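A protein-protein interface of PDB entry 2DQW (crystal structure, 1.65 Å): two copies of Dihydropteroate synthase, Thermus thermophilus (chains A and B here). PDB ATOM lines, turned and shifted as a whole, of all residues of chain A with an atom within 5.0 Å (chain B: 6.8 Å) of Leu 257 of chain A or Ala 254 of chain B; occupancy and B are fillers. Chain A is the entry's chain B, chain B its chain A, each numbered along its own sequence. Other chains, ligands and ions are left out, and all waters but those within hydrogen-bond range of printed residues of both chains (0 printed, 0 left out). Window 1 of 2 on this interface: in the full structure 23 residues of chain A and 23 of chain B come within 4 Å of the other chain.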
ATOM      1  N   SER A 252       1.006 -20.005  14.617  1.00  0.00           N
ATOM      2  CA  SER A 252      -0.398 -19.881  14.224  1.00  0.00           C
ATOM      3  C   SER A 252      -0.664 -18.463  13.735  1.00  0.00           C
ATOM      4  O   SER A 252      -1.308 -18.264  12.712  1.00  0.00           O
ATOM      5  CB  SER A 252      -1.323 -20.203  15.398  1.00  0.00           C
ATOM      6  OG  SER A 252      -1.135 -21.554  15.813  1.00  0.00           O
ATOM      7  N   VAL A 253      -0.177 -17.479  14.484  1.00  0.00           N
ATOM      8  CA  VAL A 253      -0.355 -16.086  14.070  1.00  0.00           C
ATOM      9  C   VAL A 253       0.287 -15.871  12.699  1.00  0.00           C
ATOM     10  O   VAL A 253      -0.299 -15.220  11.831  1.00  0.00           O
ATOM     11  CB  VAL A 253       0.267 -15.110  15.095  1.00  0.00           C
ATOM     12  CG1 VAL A 253       0.396 -13.708  14.484  1.00  0.00           C
ATOM     13  CG2 VAL A 253      -0.624 -15.037  16.333  1.00  0.00           C
ATOM     14  N   ALA A 254       1.481 -16.423  12.498  1.00  0.00           N
ATOM     15  CA  ALA A 254       2.175 -16.290  11.219  1.00  0.00           C
ATOM     16  C   ALA A 254       1.338 -16.872  10.075  1.00  0.00           C
ATOM     17  O   ALA A 254       1.173 -16.239   9.030  1.00  0.00           O
ATOM     18  CB  ALA A 254       3.531 -16.985  11.283  1.00  0.00           C
ATOM     19  N   ALA A 255       0.801 -18.073  10.275  1.00  0.00           N
ATOM     20  CA  ALA A 255      -0.012 -18.710   9.240  1.00  0.00           C
ATOM     21  C   ALA A 255      -1.259 -17.897   8.931  1.00  0.00           C
ATOM     22  O   ALA A 255      -1.652 -17.747   7.774  1.00  0.00           O
ATOM     23  CB  ALA A 255      -0.416 -20.119   9.681  1.00  0.00           C
ATOM     24  N   HIS A 256      -1.883 -17.384   9.982  1.00  0.00           N
ATOM     25  CA  HIS A 256      -3.090 -16.607   9.836  1.00  0.00           C
ATOM     26  C   HIS A 256      -2.837 -15.275   9.154  1.00  0.00           C
ATOM     27  O   HIS A 256      -3.663 -14.833   8.367  1.00  0.00           O
ATOM     28  CB  HIS A 256      -3.745 -16.451  11.205  1.00  0.00           C
ATOM     29  CG  HIS A 256      -4.395 -17.711  11.681  1.00  0.00           C
ATOM     30  ND1 HIS A 256      -4.650 -17.973  13.008  1.00  0.00           N
ATOM     31  CD2 HIS A 256      -4.865 -18.778  10.988  1.00  0.00           C
ATOM     32  CE1 HIS A 256      -5.250 -19.147  13.115  1.00  0.00           C
ATOM     33  NE2 HIS A 256      -5.392 -19.656  11.904  1.00  0.00           N
ATOM     34  N   LEU A 257      -1.700 -14.641   9.435  1.00  0.00           N
ATOM     35  CA  LEU A 257      -1.410 -13.375   8.759  1.00  0.00           C
ATOM     36  C   LEU A 257      -1.202 -13.650   7.272  1.00  0.00           C
ATOM     37  O   LEU A 257      -1.584 -12.846   6.419  1.00  0.00           O
ATOM     38  CB  LEU A 257      -0.175 -12.696   9.357  1.00  0.00           C
ATOM     39  CG  LEU A 257      -0.379 -12.147  10.775  1.00  0.00           C
ATOM     40  CD1 LEU A 257       0.900 -11.494  11.279  1.00  0.00           C
ATOM     41  CD2 LEU A 257      -1.530 -11.139  10.783  1.00  0.00           C
ATOM     42  N   PHE A 258      -0.599 -14.793   6.957  1.00  0.00           N
ATOM     43  CA  PHE A 258      -0.393 -15.160   5.561  1.00  0.00           C
ATOM     44  C   PHE A 258      -1.759 -15.354   4.902  1.00  0.00           C
ATOM     45  O   PHE A 258      -1.972 -14.911   3.777  1.00  0.00           O
ATOM     46  CB  PHE A 258       0.450 -16.440   5.462  1.00  0.00           C
ATOM     47  CG  PHE A 258       0.770 -16.854   4.049  1.00  0.00           C
ATOM     48  CD1 PHE A 258      -0.114 -17.647   3.320  1.00  0.00           C
ATOM     49  CD2 PHE A 258       1.960 -16.453   3.449  1.00  0.00           C
ATOM     50  CE1 PHE A 258       0.189 -18.041   2.017  1.00  0.00           C
ATOM     51  CE2 PHE A 258       2.273 -16.838   2.147  1.00  0.00           C
ATOM     52  CZ  PHE A 258       1.381 -17.637   1.428  1.00  0.00           C
ATOM     53  N   ALA A 259      -2.687 -16.002   5.606  1.00  0.00           N
ATOM     54  CA  ALA A 259      -4.030 -16.213   5.071  1.00  0.00           C
ATOM     55  C   ALA A 259      -4.717 -14.870   4.846  1.00  0.00           C
ATOM     56  O   ALA A 259      -5.434 -14.683   3.863  1.00  0.00           O
ATOM     57  CB  ALA A 259      -4.859 -17.072   6.029  1.00  0.00           C
ATOM     58  N   VAL A 260      -4.502 -13.935   5.768  1.00  0.00           N
ATOM     59  CA  VAL A 260      -5.096 -12.607   5.640  1.00  0.00           C
ATOM     60  C   VAL A 260      -4.525 -11.917   4.405  1.00  0.00           C
ATOM     61  O   VAL A 260      -5.252 -11.260   3.649  1.00  0.00           O
ATOM     62  CB  VAL A 260      -4.833 -11.774   6.915  1.00  0.00           C
ATOM     63  CG1 VAL A 260      -5.242 -10.313   6.699  1.00  0.00           C
ATOM     64  CG2 VAL A 260      -5.629 -12.369   8.067  1.00  0.00           C
ATOM     65  N   MET A 261      -3.225 -12.076   4.186  1.00  0.00           N
ATOM     66  CA  MET A 261      -2.586 -11.479   3.022  1.00  0.00           C
ATOM     67  C   MET A 261      -3.228 -12.054   1.747  1.00  0.00           C
ATOM     68  O   MET A 261      -3.345 -11.362   0.724  1.00  0.00           O
ATOM     69  CB  MET A 261      -1.084 -11.777   3.062  1.00  0.00           C
ATOM     70  CG  MET A 261      -0.288 -11.117   1.968  1.00  0.00           C
ATOM     71  SD  MET A 261       1.458 -11.550   2.051  1.00  0.00           S
ATOM     72  CE  MET A 261       1.408 -13.344   2.047  1.00  0.00           C
ATOM     73  N   ALA A 278      -1.611  -8.746  16.922  1.00  0.00           N
ATOM     74  CA  ALA A 278      -0.913  -8.904  15.651  1.00  0.00           C
ATOM     75  C   ALA A 278      -1.663  -8.209  14.516  1.00  0.00           C
ATOM     76  O   ALA A 278      -1.052  -7.570  13.657  1.00  0.00           O
ATOM     77  CB  ALA A 278      -0.733 -10.390  15.331  1.00  0.00           C
ATOM     78  N   LEU A 279      -2.988  -8.346  14.496  1.00  0.00           N
ATOM     79  CA  LEU A 279      -3.787  -7.715  13.447  1.00  0.00           C
ATOM     80  C   LEU A 279      -3.770  -6.192  13.562  1.00  0.00           C
ATOM     81  O   LEU A 279      -3.854  -5.489  12.555  1.00  0.00           O
ATOM     82  CB  LEU A 279      -5.231  -8.241  13.486  1.00  0.00           C
ATOM     83  CG  LEU A 279      -5.382  -9.668  12.955  1.00  0.00           C
ATOM     84  CD1 LEU A 279      -6.752 -10.225  13.340  1.00  0.00           C
ATOM     85  CD2 LEU A 279      -5.202  -9.667  11.427  1.00  0.00           C
ATOM     86  N   VAL A 281      -1.336  -4.390  14.203  1.00  0.00           N
ATOM     87  CA  VAL A 281      -0.152  -3.986  13.470  1.00  0.00           C
ATOM     88  C   VAL A 281      -0.315  -4.292  11.981  1.00  0.00           C
ATOM     89  O   VAL A 281      -0.178  -3.413  11.135  1.00  0.00           O
ATOM     90  CB  VAL A 281       1.121  -4.729  13.988  1.00  0.00           C
ATOM     91  CG1 VAL A 281       2.300  -4.476  13.049  1.00  0.00           C
ATOM     92  CG2 VAL A 281       1.472  -4.261  15.392  1.00  0.00           C
ATOM     93  N   TRP A 282      -0.625  -5.544  11.661  1.00  0.00           N
ATOM     94  CA  TRP A 282      -0.739  -5.946  10.268  1.00  0.00           C
ATOM     95  C   TRP A 282      -1.710  -5.133   9.426  1.00  0.00           C
ATOM     96  O   TRP A 282      -1.362  -4.686   8.334  1.00  0.00           O
ATOM     97  CB  TRP A 282      -1.106  -7.431  10.171  1.00  0.00           C
ATOM     98  CG  TRP A 282      -0.984  -7.965   8.779  1.00  0.00           C
ATOM     99  CD1 TRP A 282      -1.964  -8.029   7.828  1.00  0.00           C
ATOM    100  CD2 TRP A 282       0.203  -8.482   8.167  1.00  0.00           C
ATOM    101  NE1 TRP A 282      -1.458  -8.548   6.657  1.00  0.00           N
ATOM    102  CE2 TRP A 282      -0.126  -8.824   6.836  1.00  0.00           C
ATOM    103  CE3 TRP A 282       1.521  -8.664   8.607  1.00  0.00           C
ATOM    104  CZ2 TRP A 282       0.810  -9.368   5.946  1.00  0.00           C
ATOM    105  CZ3 TRP A 282       2.453  -9.206   7.723  1.00  0.00           C
ATOM    106  CH2 TRP A 282       2.090  -9.538   6.404  1.00  0.00           C
ATOM    107  N   ILE B 236       4.852  -0.387  17.960  1.00  0.00           N
ATOM    108  CA  ILE B 236       4.150  -1.632  18.231  1.00  0.00           C
ATOM    109  C   ILE B 236       3.110  -1.433  19.332  1.00  0.00           C
ATOM    110  O   ILE B 236       1.990  -1.934  19.237  1.00  0.00           O
ATOM    111  CB  ILE B 236       5.125  -2.747  18.649  1.00  0.00           C
ATOM    112  CG1 ILE B 236       6.204  -2.927  17.576  1.00  0.00           C
ATOM    113  CG2 ILE B 236       4.354  -4.050  18.867  1.00  0.00           C
ATOM    114  CD1 ILE B 236       5.663  -3.214  16.179  1.00  0.00           C
ATOM    115  N   VAL B 249       5.352  -8.863  22.135  1.00  0.00           N
ATOM    116  CA  VAL B 249       5.856  -9.843  21.177  1.00  0.00           C
ATOM    117  C   VAL B 249       4.971 -10.099  19.960  1.00  0.00           C
ATOM    118  O   VAL B 249       5.474 -10.203  18.843  1.00  0.00           O
ATOM    119  CB  VAL B 249       6.175 -11.203  21.862  1.00  0.00           C
ATOM    120  CG1 VAL B 249       4.899 -11.852  22.394  1.00  0.00           C
ATOM    121  CG2 VAL B 249       6.886 -12.128  20.871  1.00  0.00           C
ATOM    122  N   HIS B 250       3.660 -10.194  20.150  1.00  0.00           N
ATOM    123  CA  HIS B 250       2.805 -10.508  19.005  1.00  0.00           C
ATOM    124  C   HIS B 250       2.771  -9.369  17.976  1.00  0.00           C
ATOM    125  O   HIS B 250       2.803  -9.585  16.772  1.00  0.00           O
ATOM    126  CB  HIS B 250       1.394 -10.782  19.526  1.00  0.00           C
ATOM    127  CG  HIS B 250       1.391 -12.061  20.322  1.00  0.00           C
ATOM    128  ND1 HIS B 250       1.803 -13.251  19.820  1.00  0.00           N
ATOM    129  CD2 HIS B 250       0.991 -12.254  21.648  1.00  0.00           C
ATOM    130  CE1 HIS B 250       1.658 -14.138  20.823  1.00  0.00           C
ATOM    131  NE2 HIS B 250       1.173 -13.569  21.929  1.00  0.00           N
ATOM    132  N   GLY B 251       2.737  -8.124  18.431  1.00  0.00           N
ATOM    133  CA  GLY B 251       2.748  -7.029  17.480  1.00  0.00           C
ATOM    134  C   GLY B 251       4.112  -6.903  16.819  1.00  0.00           C
ATOM    135  O   GLY B 251       4.204  -6.526  15.652  1.00  0.00           O
ATOM    136  N   SER B 252       5.174  -7.210  17.563  1.00  0.00           N
ATOM    137  CA  SER B 252       6.528  -7.132  17.022  1.00  0.00           C
ATOM    138  C   SER B 252       6.717  -8.187  15.936  1.00  0.00           C
ATOM    139  O   SER B 252       7.281  -7.913  14.878  1.00  0.00           O
ATOM    140  CB  SER B 252       7.563  -7.334  18.133  1.00  0.00           C
ATOM    141  OG  SER B 252       7.460  -6.300  19.104  1.00  0.00           O
ATOM    142  N   VAL B 253       6.238  -9.396  16.199  1.00  0.00           N
ATOM    143  CA  VAL B 253       6.358 -10.455  15.208  1.00  0.00           C
ATOM    144  C   VAL B 253       5.594 -10.062  13.949  1.00  0.00           C
ATOM    145  O   VAL B 253       6.079 -10.257  12.838  1.00  0.00           O
ATOM    146  CB  VAL B 253       5.813 -11.789  15.752  1.00  0.00           C
ATOM    147  CG1 VAL B 253       5.647 -12.792  14.621  1.00  0.00           C
ATOM    148  CG2 VAL B 253       6.770 -12.337  16.795  1.00  0.00           C
ATOM    149  N   ALA B 254       4.403  -9.489  14.120  1.00  0.00           N
ATOM    150  CA  ALA B 254       3.605  -9.075  12.970  1.00  0.00           C
ATOM    151  C   ALA B 254       4.344  -8.023  12.135  1.00  0.00           C
ATOM    152  O   ALA B 254       4.390  -8.116  10.909  1.00  0.00           O
ATOM    153  CB  ALA B 254       2.248  -8.524  13.437  1.00  0.00           C
ATOM    154  N   ALA B 255       4.931  -7.027  12.798  1.00  0.00           N
ATOM    155  CA  ALA B 255       5.647  -5.976  12.069  1.00  0.00           C
ATOM    156  C   ALA B 255       6.858  -6.534  11.349  1.00  0.00           C
ATOM    157  O   ALA B 255       7.169  -6.139  10.219  1.00  0.00           O
ATOM    158  CB  ALA B 255       6.089  -4.868  13.026  1.00  0.00           C
ATOM    159  N   HIS B 256       7.539  -7.462  12.011  1.00  0.00           N
ATOM    160  CA  HIS B 256       8.725  -8.064  11.441  1.00  0.00           C
ATOM    161  C   HIS B 256       8.387  -8.969  10.267  1.00  0.00           C
ATOM    162  O   HIS B 256       9.125  -8.993   9.287  1.00  0.00           O
ATOM    163  CB  HIS B 256       9.504  -8.789  12.537  1.00  0.00           C
ATOM    164  CG  HIS B 256      10.253  -7.852  13.440  1.00  0.00           C
ATOM    165  ND1 HIS B 256      10.619  -8.185  14.726  1.00  0.00           N
ATOM    166  CD2 HIS B 256      10.709  -6.593  13.231  1.00  0.00           C
ATOM    167  CE1 HIS B 256      11.269  -7.170  15.272  1.00  0.00           C
ATOM    168  NE2 HIS B 256      11.337  -6.192  14.384  1.00  0.00           N
ATOM    169  N   LEU B 257       7.272  -9.694  10.341  1.00  0.00           N
ATOM    170  CA  LEU B 257       6.894 -10.533   9.207  1.00  0.00           C
ATOM    171  C   LEU B 257       6.568  -9.625   8.023  1.00  0.00           C
ATOM    172  O   LEU B 257       6.838  -9.968   6.884  1.00  0.00           O
ATOM    173  CB  LEU B 257       5.690 -11.416   9.542  1.00  0.00           C
ATOM    174  CG  LEU B 257       6.011 -12.533  10.541  1.00  0.00           C
ATOM    175  CD1 LEU B 257       4.758 -13.346  10.796  1.00  0.00           C
ATOM    176  CD2 LEU B 257       7.128 -13.426   9.984  1.00  0.00           C
ATOM    177  N   PHE B 258       6.000  -8.454   8.295  1.00  0.00           N
ATOM    178  CA  PHE B 258       5.681  -7.526   7.212  1.00  0.00           C
ATOM    179  C   PHE B 258       6.988  -7.041   6.585  1.00  0.00           C
ATOM    180  O   PHE B 258       7.096  -6.934   5.363  1.00  0.00           O
ATOM    181  CB  PHE B 258       4.855  -6.342   7.747  1.00  0.00           C
ATOM    182  CG  PHE B 258       4.397  -5.386   6.679  1.00  0.00           C
ATOM    183  CD1 PHE B 258       5.183  -4.299   6.318  1.00  0.00           C
ATOM    184  CD2 PHE B 258       3.184  -5.584   6.022  1.00  0.00           C
ATOM    185  CE1 PHE B 258       4.770  -3.426   5.315  1.00  0.00           C
ATOM    186  CE2 PHE B 258       2.764  -4.717   5.016  1.00  0.00           C
ATOM    187  CZ  PHE B 258       3.562  -3.634   4.668  1.00  0.00           C
ATOM    188  N   ALA B 259       7.986  -6.757   7.419  1.00  0.00           N
ATOM    189  CA  ALA B 259       9.280  -6.304   6.913  1.00  0.00           C
ATOM    190  C   ALA B 259       9.908  -7.400   6.053  1.00  0.00           C
ATOM    191  O   ALA B 259      10.522  -7.123   5.024  1.00  0.00           O
ATOM    192  CB  ALA B 259      10.204  -5.952   8.071  1.00  0.00           C
ATOM    193  N   HIS B 275      10.273 -15.468  17.173  1.00  0.00           N
ATOM    194  CA  HIS B 275      10.524 -15.158  15.773  1.00  0.00           C
ATOM    195  C   HIS B 275      10.945 -16.390  14.973  1.00  0.00           C
ATOM    196  O   HIS B 275      10.532 -16.547  13.826  1.00  0.00           O
ATOM    197  CB  HIS B 275      11.560 -14.038  15.652  1.00  0.00           C
ATOM    198  CG  HIS B 275      11.003 -12.678  15.945  1.00  0.00           C
ATOM    199  ND1 HIS B 275      10.867 -12.187  17.225  1.00  0.00           N
ATOM    200  CD2 HIS B 275      10.512 -11.720  15.120  1.00  0.00           C
ATOM    201  CE1 HIS B 275      10.318 -10.984  17.177  1.00  0.00           C
ATOM    202  NE2 HIS B 275      10.090 -10.678  15.911  1.00  0.00           N
ATOM    203  N   TRP B 282       6.236 -18.813   8.204  1.00  0.00           N
ATOM    204  CA  TRP B 282       6.251 -17.814   7.141  1.00  0.00           C
ATOM    205  C   TRP B 282       7.142 -18.152   5.953  1.00  0.00           C
ATOM    206  O   TRP B 282       6.703 -18.089   4.798  1.00  0.00           O
ATOM    207  CB  TRP B 282       6.648 -16.449   7.714  1.00  0.00           C
ATOM    208  CG  TRP B 282       6.418 -15.333   6.747  1.00  0.00           C
ATOM    209  CD1 TRP B 282       7.314 -14.815   5.855  1.00  0.00           C
ATOM    210  CD2 TRP B 282       5.189 -14.632   6.543  1.00  0.00           C
ATOM    211  NE1 TRP B 282       6.711 -13.827   5.103  1.00  0.00           N
ATOM    212  CE2 TRP B 282       5.407 -13.699   5.506  1.00  0.00           C
ATOM    213  CE3 TRP B 282       3.921 -14.705   7.136  1.00  0.00           C
ATOM    214  CZ2 TRP B 282       4.400 -12.841   5.047  1.00  0.00           C
ATOM    215  CZ3 TRP B 282       2.921 -13.855   6.683  1.00  0.00           C
ATOM    216  CH2 TRP B 282       3.167 -12.933   5.646  1.00  0.00           C
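Among the printed residues, merely in contact across the chains: Ala 278 of chain A with Ala 254 of chain B (3.4 Å), Val 281 of chain A with Gly 251 of chain B (3.6 Å), Trp 282 of chain A with Trp 282 of chain B (3.6 Å), Phe 258 of chain A with Trp 282 of chain B (3.7 Å), Trp 282 of chain A with Phe 258 of chain B (3.7 Å), Ala 254 of chain A with Trp 282 of chain B (3.7 Å), Val 281 of chain A with Ala 255 of chain B (3.7 Å), Trp 282 of chain A with Ala 254 of chain B (3.7 Å), Ala 254 of chain A with Leu 257 of chain B (3.9 Å), Ala 278 of chain A with His 250 of chain B (3.9 Å), Leu 257 of chain A with Ala 254 of chain B (3.9 Å) and Val 281 of chain A with Ala 254 of chain B (3.997 Å).
Of chain B, only Ala 254 (3.9 Å) comes within 4 Å of Leu 257 of chain A. Of the printed residues of chain A, Ala 254 of chain B touches Leu 257, Ala 278, Val 281 and Trp 282. Printed residues of chain A within 4 Å of Trp 282 of chain B: Ala 254 (3.7 Å), Phe 258 (3.7 Å) and Trp 282 (3.6 Å). Printed residues of chain B within 4 Å of Phe 258 of chain A: Trp 282. Of the printed residues of chain A, His 250 of chain B touches Ala 278. Printed residues of chain A within 4 Å of Gly 251 of chain B: Val 281. Leu 279 of chain A touches none of the printed residues of chain B. Ser 252 of chain A touches none of the printed residues of chain B. The nearest residue of chain B that does not touch Leu 257 of chain A is Trp 282 of chain B (4.2 Å).
Of the 14 printed residues of chain A, 6 touch a printed residue of chain B. Hydrophobic or aromatic side chains of chain A that line the printed part of chain B: Ala 254, Leu 257, Phe 258, Ala 278, Val 281 and Trp 282. Of the 14 printed residues of chain B, 7 touch a printed residue of chain A. Printed residues of chain B that touch a printed residue of chain A: His 250, Gly 251, Ala 254, Ala 255, Leu 257, Phe 258 and Trp 282. Among the printed residues, no Asp or Glu carboxylate lies within 4 Å of a Lys or Arg side-chain nitrogen of the other chain.
Ala 254 of chain A touches Leu 257 of chain B, and with the chains exchanged Leu 257 of chain A touches Ala 254 of chain B. Ala 254 of chain A touches Trp 282 of chain B, and with the chains exchanged Trp 282 of chain A touches Ala 254 of chain B. Phe 258 of chain A touches Trp 282 of chain B, and with the chains exchanged Trp 282 of chain A touches Phe 258 of chain B. Trp 282 of chain A touches its own counterpart, Trp 282 of chain B.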
